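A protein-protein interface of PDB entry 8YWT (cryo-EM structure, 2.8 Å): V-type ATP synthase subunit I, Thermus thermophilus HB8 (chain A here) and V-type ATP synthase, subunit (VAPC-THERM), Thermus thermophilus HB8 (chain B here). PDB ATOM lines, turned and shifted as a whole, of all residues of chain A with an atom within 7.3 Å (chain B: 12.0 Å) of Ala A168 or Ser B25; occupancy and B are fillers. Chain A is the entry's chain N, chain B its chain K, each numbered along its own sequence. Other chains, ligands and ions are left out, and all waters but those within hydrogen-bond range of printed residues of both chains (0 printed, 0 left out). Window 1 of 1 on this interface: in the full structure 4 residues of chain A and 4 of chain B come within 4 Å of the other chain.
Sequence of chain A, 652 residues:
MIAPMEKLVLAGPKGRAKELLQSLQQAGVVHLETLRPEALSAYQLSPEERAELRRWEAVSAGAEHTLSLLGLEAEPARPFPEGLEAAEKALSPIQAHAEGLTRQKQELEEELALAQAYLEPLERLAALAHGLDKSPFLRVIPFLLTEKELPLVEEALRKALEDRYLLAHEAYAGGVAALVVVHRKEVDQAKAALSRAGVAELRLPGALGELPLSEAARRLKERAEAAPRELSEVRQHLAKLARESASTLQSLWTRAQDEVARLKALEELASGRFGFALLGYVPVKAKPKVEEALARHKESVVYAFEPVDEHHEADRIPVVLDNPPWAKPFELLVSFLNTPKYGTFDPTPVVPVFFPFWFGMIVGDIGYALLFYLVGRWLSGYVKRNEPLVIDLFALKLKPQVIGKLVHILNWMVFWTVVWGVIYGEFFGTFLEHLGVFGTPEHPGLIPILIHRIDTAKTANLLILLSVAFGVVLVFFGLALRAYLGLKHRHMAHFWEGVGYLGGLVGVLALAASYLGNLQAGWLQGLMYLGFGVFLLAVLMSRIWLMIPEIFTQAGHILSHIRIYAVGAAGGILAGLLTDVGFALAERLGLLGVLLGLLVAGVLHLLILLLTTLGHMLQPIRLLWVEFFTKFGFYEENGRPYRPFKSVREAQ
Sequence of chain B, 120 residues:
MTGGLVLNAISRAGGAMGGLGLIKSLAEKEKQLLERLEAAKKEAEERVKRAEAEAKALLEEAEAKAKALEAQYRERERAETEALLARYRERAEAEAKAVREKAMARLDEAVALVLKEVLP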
ATOM      1  N   ALA A 127      15.831  16.842 -12.401  1.00  0.00           N
ATOM      2  CA  ALA A 127      16.047  15.930 -13.526  1.00  0.00           C
ATOM      3  C   ALA A 127      17.526  15.817 -13.949  1.00  0.00           C
ATOM      4  O   ALA A 127      17.941  14.794 -14.490  1.00  0.00           O
ATOM      5  CB  ALA A 127      15.187  16.419 -14.694  1.00  0.00           C
ATOM      6  N   LEU A 128      18.322  16.863 -13.718  1.00  0.00           N
ATOM      7  CA  LEU A 128      19.774  16.893 -13.932  1.00  0.00           C
ATOM      8  C   LEU A 128      20.514  16.077 -12.860  1.00  0.00           C
ATOM      9  O   LEU A 128      21.523  15.435 -13.145  1.00  0.00           O
ATOM     10  CB  LEU A 128      20.195  18.372 -13.931  1.00  0.00           C
ATOM     11  CG  LEU A 128      21.666  18.679 -14.229  1.00  0.00           C
ATOM     12  CD1 LEU A 128      22.094  18.197 -15.607  1.00  0.00           C
ATOM     13  CD2 LEU A 128      21.872  20.190 -14.174  1.00  0.00           C
ATOM     14  N   ALA A 129      19.988  16.067 -11.635  1.00  0.00           N
ATOM     15  CA  ALA A 129      20.335  15.125 -10.582  1.00  0.00           C
ATOM     16  C   ALA A 129      19.726  13.728 -10.834  1.00  0.00           C
ATOM     17  O   ALA A 129      18.677  13.595 -11.465  1.00  0.00           O
ATOM     18  CB  ALA A 129      19.836  15.709  -9.253  1.00  0.00           C
ATOM     19  N   HIS A 130      20.345  12.688 -10.268  1.00  0.00           N
ATOM     20  CA  HIS A 130      19.868  11.291 -10.310  1.00  0.00           C
ATOM     21  C   HIS A 130      19.656  10.705  -8.903  1.00  0.00           C
ATOM     22  O   HIS A 130      19.906   9.523  -8.664  1.00  0.00           O
ATOM     23  CB  HIS A 130      20.809  10.427 -11.168  1.00  0.00           C
ATOM     24  CG  HIS A 130      21.136  11.006 -12.520  1.00  0.00           C
ATOM     25  ND1 HIS A 130      20.283  11.030 -13.627  1.00  0.00           N
ATOM     26  CD2 HIS A 130      22.324  11.575 -12.865  1.00  0.00           C
ATOM     27  CE1 HIS A 130      20.981  11.615 -14.615  1.00  0.00           C
ATOM     28  NE2 HIS A 130      22.208  11.942 -14.185  1.00  0.00           N
ATOM     29  N   LEU A 132      21.560  11.980  -6.387  1.00  0.00           N
ATOM     30  CA  LEU A 132      22.879  12.202  -5.782  1.00  0.00           C
ATOM     31  C   LEU A 132      22.814  13.109  -4.539  1.00  0.00           C
ATOM     32  O   LEU A 132      23.677  12.994  -3.673  1.00  0.00           O
ATOM     33  CB  LEU A 132      23.873  12.778  -6.809  1.00  0.00           C
ATOM     34  CG  LEU A 132      24.555  11.729  -7.708  1.00  0.00           C
ATOM     35  CD1 LEU A 132      23.617  11.097  -8.726  1.00  0.00           C
ATOM     36  CD2 LEU A 132      25.702  12.375  -8.474  1.00  0.00           C
ATOM     37  N   ILE A 141      25.743  20.983  -5.084  1.00  0.00           N
ATOM     38  CA  ILE A 141      25.473  22.430  -5.031  1.00  0.00           C
ATOM     39  C   ILE A 141      24.686  22.865  -6.288  1.00  0.00           C
ATOM     40  O   ILE A 141      25.237  22.811  -7.393  1.00  0.00           O
ATOM     41  CB  ILE A 141      26.781  23.240  -4.885  1.00  0.00           C
ATOM     42  CG1 ILE A 141      27.647  22.838  -3.669  1.00  0.00           C
ATOM     43  CG2 ILE A 141      26.479  24.749  -4.845  1.00  0.00           C
ATOM     44  CD1 ILE A 141      27.027  23.101  -2.294  1.00  0.00           C
ATOM     45  N   PHE A 143      22.954  25.776  -8.773  1.00  0.00           N
ATOM     46  CA  PHE A 143      23.026  27.197  -9.157  1.00  0.00           C
ATOM     47  C   PHE A 143      22.573  27.436 -10.609  1.00  0.00           C
ATOM     48  O   PHE A 143      22.419  26.504 -11.395  1.00  0.00           O
ATOM     49  CB  PHE A 143      24.432  27.769  -8.897  1.00  0.00           C
ATOM     50  CG  PHE A 143      25.563  27.127  -9.668  1.00  0.00           C
ATOM     51  CD1 PHE A 143      26.136  25.936  -9.196  1.00  0.00           C
ATOM     52  CD2 PHE A 143      26.057  27.727 -10.841  1.00  0.00           C
ATOM     53  CE1 PHE A 143      27.185  25.332  -9.903  1.00  0.00           C
ATOM     54  CE2 PHE A 143      27.122  27.130 -11.537  1.00  0.00           C
ATOM     55  CZ  PHE A 143      27.682  25.929 -11.070  1.00  0.00           C
ATOM     56  N   LEU A 150      30.362  30.111 -17.917  1.00  0.00           N
ATOM     57  CA  LEU A 150      30.608  28.762 -17.388  1.00  0.00           C
ATOM     58  C   LEU A 150      32.107  28.362 -17.300  1.00  0.00           C
ATOM     59  O   LEU A 150      32.500  27.780 -16.286  1.00  0.00           O
ATOM     60  CB  LEU A 150      29.739  27.775 -18.191  1.00  0.00           C
ATOM     61  CG  LEU A 150      29.817  26.313 -17.729  1.00  0.00           C
ATOM     62  CD1 LEU A 150      29.329  26.121 -16.294  1.00  0.00           C
ATOM     63  CD2 LEU A 150      28.935  25.467 -18.637  1.00  0.00           C
ATOM     64  N   LEU A 166      32.621  17.264  -9.904  1.00  0.00           N
ATOM     65  CA  LEU A 166      31.889  17.167 -11.167  1.00  0.00           C
ATOM     66  C   LEU A 166      31.004  18.411 -11.334  1.00  0.00           C
ATOM     67  O   LEU A 166      30.676  19.071 -10.348  1.00  0.00           O
ATOM     68  CB  LEU A 166      31.044  15.878 -11.255  1.00  0.00           C
ATOM     69  CG  LEU A 166      31.784  14.546 -11.026  1.00  0.00           C
ATOM     70  CD1 LEU A 166      31.783  14.114  -9.560  1.00  0.00           C
ATOM     71  CD2 LEU A 166      31.114  13.426 -11.817  1.00  0.00           C
ATOM     72  N   LEU A 167      30.604  18.725 -12.567  1.00  0.00           N
ATOM     73  CA  LEU A 167      29.726  19.853 -12.891  1.00  0.00           C
ATOM     74  C   LEU A 167      28.846  19.501 -14.096  1.00  0.00           C
ATOM     75  O   LEU A 167      29.248  19.665 -15.247  1.00  0.00           O
ATOM     76  CB  LEU A 167      30.586  21.121 -13.080  1.00  0.00           C
ATOM     77  CG  LEU A 167      29.875  22.354 -13.678  1.00  0.00           C
ATOM     78  CD1 LEU A 167      28.515  22.651 -13.046  1.00  0.00           C
ATOM     79  CD2 LEU A 167      30.759  23.584 -13.476  1.00  0.00           C
ATOM     80  N   ALA A 168      27.646  18.993 -13.822  1.00  0.00           N
ATOM     81  CA  ALA A 168      26.627  18.734 -14.839  1.00  0.00           C
ATOM     82  C   ALA A 168      25.795  19.998 -15.126  1.00  0.00           C
ATOM     83  O   ALA A 168      25.549  20.798 -14.222  1.00  0.00           O
ATOM     84  CB  ALA A 168      25.758  17.564 -14.375  1.00  0.00           C
ATOM     85  N   HIS A 169      25.334  20.181 -16.364  1.00  0.00           N
ATOM     86  CA  HIS A 169      24.517  21.344 -16.726  1.00  0.00           C
ATOM     87  C   HIS A 169      23.520  21.081 -17.861  1.00  0.00           C
ATOM     88  O   HIS A 169      23.699  20.170 -18.669  1.00  0.00           O
ATOM     89  CB  HIS A 169      25.426  22.543 -17.030  1.00  0.00           C
ATOM     90  CG  HIS A 169      26.310  22.384 -18.241  1.00  0.00           C
ATOM     91  ND1 HIS A 169      25.929  22.635 -19.562  1.00  0.00           N
ATOM     92  CD2 HIS A 169      27.609  21.974 -18.226  1.00  0.00           C
ATOM     93  CE1 HIS A 169      27.014  22.381 -20.312  1.00  0.00           C
ATOM     94  NE2 HIS A 169      28.034  21.977 -19.536  1.00  0.00           N
ATOM     95  N   GLU A 170      22.472  21.902 -17.935  1.00  0.00           N
ATOM     96  CA  GLU A 170      21.501  21.925 -19.037  1.00  0.00           C
ATOM     97  C   GLU A 170      21.042  23.358 -19.362  1.00  0.00           C
ATOM     98  O   GLU A 170      20.696  24.128 -18.470  1.00  0.00           O
ATOM     99  CB  GLU A 170      20.307  21.016 -18.697  1.00  0.00           C
ATOM    100  CG  GLU A 170      19.222  21.052 -19.782  1.00  0.00           C
ATOM    101  CD  GLU A 170      18.095  20.037 -19.550  1.00  0.00           C
ATOM    102  OE1 GLU A 170      17.787  19.711 -18.385  1.00  0.00           O
ATOM    103  OE2 GLU A 170      17.495  19.570 -20.547  1.00  0.00           O
ATOM    104  N   VAL A 176      21.228  28.692 -17.985  1.00  0.00           N
ATOM    105  CA  VAL A 176      21.747  27.345 -17.732  1.00  0.00           C
ATOM    106  C   VAL A 176      21.435  26.924 -16.301  1.00  0.00           C
ATOM    107  O   VAL A 176      21.719  27.659 -15.359  1.00  0.00           O
ATOM    108  CB  VAL A 176      23.265  27.292 -17.988  1.00  0.00           C
ATOM    109  CG1 VAL A 176      23.877  25.935 -17.637  1.00  0.00           C
ATOM    110  CG2 VAL A 176      23.597  27.573 -19.453  1.00  0.00           C
ATOM    111  N   ALA A 177      20.905  25.716 -16.145  1.00  0.00           N
ATOM    112  CA  ALA A 177      20.784  24.998 -14.886  1.00  0.00           C
ATOM    113  C   ALA A 177      22.093  24.248 -14.626  1.00  0.00           C
ATOM    114  O   ALA A 177      22.517  23.467 -15.475  1.00  0.00           O
ATOM    115  CB  ALA A 177      19.604  24.027 -15.017  1.00  0.00           C
ATOM    116  N   ALA A 178      22.744  24.485 -13.490  1.00  0.00           N
ATOM    117  CA  ALA A 178      24.070  23.949 -13.189  1.00  0.00           C
ATOM    118  C   ALA A 178      24.128  23.254 -11.816  1.00  0.00           C
ATOM    119  O   ALA A 178      23.448  23.638 -10.863  1.00  0.00           O
ATOM    120  CB  ALA A 178      25.089  25.081 -13.320  1.00  0.00           C
ATOM    121  N   LEU A 179      24.933  22.195 -11.736  1.00  0.00           N
ATOM    122  CA  LEU A 179      24.915  21.246 -10.627  1.00  0.00           C
ATOM    123  C   LEU A 179      26.336  20.744 -10.320  1.00  0.00           C
ATOM    124  O   LEU A 179      26.809  19.782 -10.926  1.00  0.00           O
ATOM    125  CB  LEU A 179      23.934  20.126 -11.033  1.00  0.00           C
ATOM    126  CG  LEU A 179      23.470  19.246  -9.868  1.00  0.00           C
ATOM    127  CD1 LEU A 179      22.440  19.988  -9.011  1.00  0.00           C
ATOM    128  CD2 LEU A 179      22.805  17.982 -10.398  1.00  0.00           C
ATOM    129  N   VAL A 180      27.033  21.415  -9.397  1.00  0.00           N
ATOM    130  CA  VAL A 180      28.334  20.956  -8.875  1.00  0.00           C
ATOM    131  C   VAL A 180      28.129  19.756  -7.957  1.00  0.00           C
ATOM    132  O   VAL A 180      27.189  19.737  -7.163  1.00  0.00           O
ATOM    133  CB  VAL A 180      29.099  22.096  -8.163  1.00  0.00           C
ATOM    134  CG1 VAL A 180      30.044  21.672  -7.029  1.00  0.00           C
ATOM    135  CG2 VAL A 180      29.981  22.839  -9.168  1.00  0.00           C
ATOM    136  N   VAL A 181      29.038  18.784  -8.007  1.00  0.00           N
ATOM    137  CA  VAL A 181      29.084  17.633  -7.092  1.00  0.00           C
ATOM    138  C   VAL A 181      30.498  17.492  -6.525  1.00  0.00           C
ATOM    139  O   VAL A 181      31.463  17.525  -7.286  1.00  0.00           O
ATOM    140  CB  VAL A 181      28.639  16.338  -7.798  1.00  0.00           C
ATOM    141  CG1 VAL A 181      28.525  15.174  -6.814  1.00  0.00           C
ATOM    142  CG2 VAL A 181      27.295  16.490  -8.526  1.00  0.00           C
ATOM    143  N   GLY B  21      27.258  18.387 -18.398  1.00  0.00           N
ATOM    144  CA  GLY B  21      26.636  18.837 -19.635  1.00  0.00           C
ATOM    145  C   GLY B  21      25.559  17.894 -20.177  1.00  0.00           C
ATOM    146  O   GLY B  21      25.089  16.990 -19.482  1.00  0.00           O
ATOM    147  N   LEU B  22      25.201  18.051 -21.452  1.00  0.00           N
ATOM    148  CA  LEU B  22      24.243  17.166 -22.120  1.00  0.00           C
ATOM    149  C   LEU B  22      24.687  15.692 -22.189  1.00  0.00           C
ATOM    150  O   LEU B  22      23.855  14.786 -22.094  1.00  0.00           O
ATOM    151  N   ILE B  23      25.996  15.436 -22.270  1.00  0.00           N
ATOM    152  CA  ILE B  23      26.568  14.127 -21.975  1.00  0.00           C
ATOM    153  C   ILE B  23      27.187  14.007 -20.570  1.00  0.00           C
ATOM    154  O   ILE B  23      27.203  12.922 -19.987  1.00  0.00           O
ATOM    155  N   LYS B  24      27.657  15.107 -19.972  1.00  0.00           N
ATOM    156  CA  LYS B  24      28.287  15.101 -18.652  1.00  0.00           C
ATOM    157  C   LYS B  24      27.351  14.742 -17.487  1.00  0.00           C
ATOM    158  O   LYS B  24      27.780  14.114 -16.517  1.00  0.00           O
ATOM    159  N   SER B  25      26.055  15.039 -17.599  1.00  0.00           N
ATOM    160  CA  SER B  25      25.044  14.550 -16.670  1.00  0.00           C
ATOM    161  C   SER B  25      24.880  13.021 -16.698  1.00  0.00           C
ATOM    162  O   SER B  25      24.640  12.410 -15.655  1.00  0.00           O
ATOM    163  N   LEU B  26      25.087  12.377 -17.850  1.00  0.00           N
ATOM    164  CA  LEU B  26      25.101  10.922 -17.974  1.00  0.00           C
ATOM    165  C   LEU B  26      26.375  10.263 -17.416  1.00  0.00           C
ATOM    166  O   LEU B  26      26.305   9.194 -16.804  1.00  0.00           O
ATOM    167  N   ALA B  27      27.532  10.921 -17.542  1.00  0.00           N
ATOM    168  CA  ALA B  27      28.776  10.482 -16.909  1.00  0.00           C
ATOM    169  C   ALA B  27      28.731  10.537 -15.371  1.00  0.00           C
ATOM    170  O   ALA B  27      29.115   9.576 -14.701  1.00  0.00           O
ATOM    171  N   GLU B  28      28.171  11.605 -14.796  1.00  0.00           N
ATOM    172  CA  GLU B  28      27.872  11.659 -13.367  1.00  0.00           C
ATOM    173  C   GLU B  28      26.759  10.687 -12.929  1.00  0.00           C
ATOM    174  O   GLU B  28      26.828  10.119 -11.837  1.00  0.00           O
ATOM    175  N   LYS B  29      25.774  10.421 -13.793  1.00  0.00           N
ATOM    176  CA  LYS B  29      24.736   9.422 -13.555  1.00  0.00           C
ATOM    177  C   LYS B  29      25.277   7.991 -13.434  1.00  0.00           C
ATOM    178  O   LYS B  29      24.866   7.247 -12.540  1.00  0.00           O
ATOM    179  N   GLU B  30      26.262   7.618 -14.254  1.00  0.00           N
ATOM    180  CA  GLU B  30      27.002   6.373 -14.074  1.00  0.00           C
ATOM    181  C   GLU B  30      27.859   6.365 -12.797  1.00  0.00           C
ATOM    182  O   GLU B  30      27.898   5.365 -12.074  1.00  0.00           O
ATOM    183  N   LYS B  31      28.484   7.495 -12.456  1.00  0.00           N
ATOM    184  CA  LYS B  31      29.260   7.646 -11.228  1.00  0.00           C
ATOM    185  C   LYS B  31      28.442   7.526  -9.931  1.00  0.00           C
ATOM    186  O   LYS B  31      28.962   7.064  -8.912  1.00  0.00           O
ATOM    187  N   GLN B  32      27.148   7.849  -9.963  1.00  0.00           N
ATOM    188  CA  GLN B  32      26.233   7.628  -8.842  1.00  0.00           C
ATOM    189  C   GLN B  32      25.988   6.148  -8.491  1.00  0.00           C
ATOM    190  O   GLN B  32      25.570   5.835  -7.372  1.00  0.00           O
ATOM    191  N   LEU B  33      26.321   5.220  -9.392  1.00  0.00           N
ATOM    192  CA  LEU B  33      26.286   3.786  -9.124  1.00  0.00           C
ATOM    193  C   LEU B  33      27.252   3.315  -8.023  1.00  0.00           C
ATOM    194  O   LEU B  33      26.984   2.307  -7.366  1.00  0.00           O
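NE2 of His A130 is in hydrogen-bond range of O of Ser B25.
The backbone NH of His A169 lies close to the backbone NH of Gly B21, at 3.3 Å.
O of Ala A168 lies within hydrogen-bond range of N of Leu A179 (2.9 Å).
Among the printed residues, pairs that only touch across the chains: His A130 with Lys B29 (3.3 Å), Ala A168 with Gly B21 (3.6 Å), His A169 with Leu B22 (3.8 Å), Ala A168 with Ser B25 (3.9 Å) and Leu A167 with Gly B21 (3.9 Å).
No residue of chain B comes within 4 Å of Leu A128.
Printed residues of chain B within 4 Å of His A130: Ser B25 (2.9 Å) and Lys B29 (3.3 Å).
Leu A167 touches just one residue of chain B: Gly B21.
Of the printed residues of chain B, Ala A168 touches Gly B21 (3.6 Å) and Ser B25 (3.9 Å).
Of chain B, only Gly B21 and Leu B22 come within 4 Å of His A169.
No residue of chain B comes within 4 Å of Ala A178.
No residue of chain B comes within 4 Å of Leu A179.
Of the printed residues of chain A, Gly B21 touches Leu A167, Ala A168 and His A169.
Of the printed residues of chain A, Leu B22 touches His A169 (3.8 Å).
No residue of chain A comes within 4 Å of Lys B24.
Ser B25 touches just these residues of chain A: His A130 and Ala A168.
Printed residues of chain A within 4 Å of Lys B29: His A130 (3.3 Å).
Hydrophobic or aromatic side chains of chain A that line the printed part of chain B: His A130, Ala A168 and His A169.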
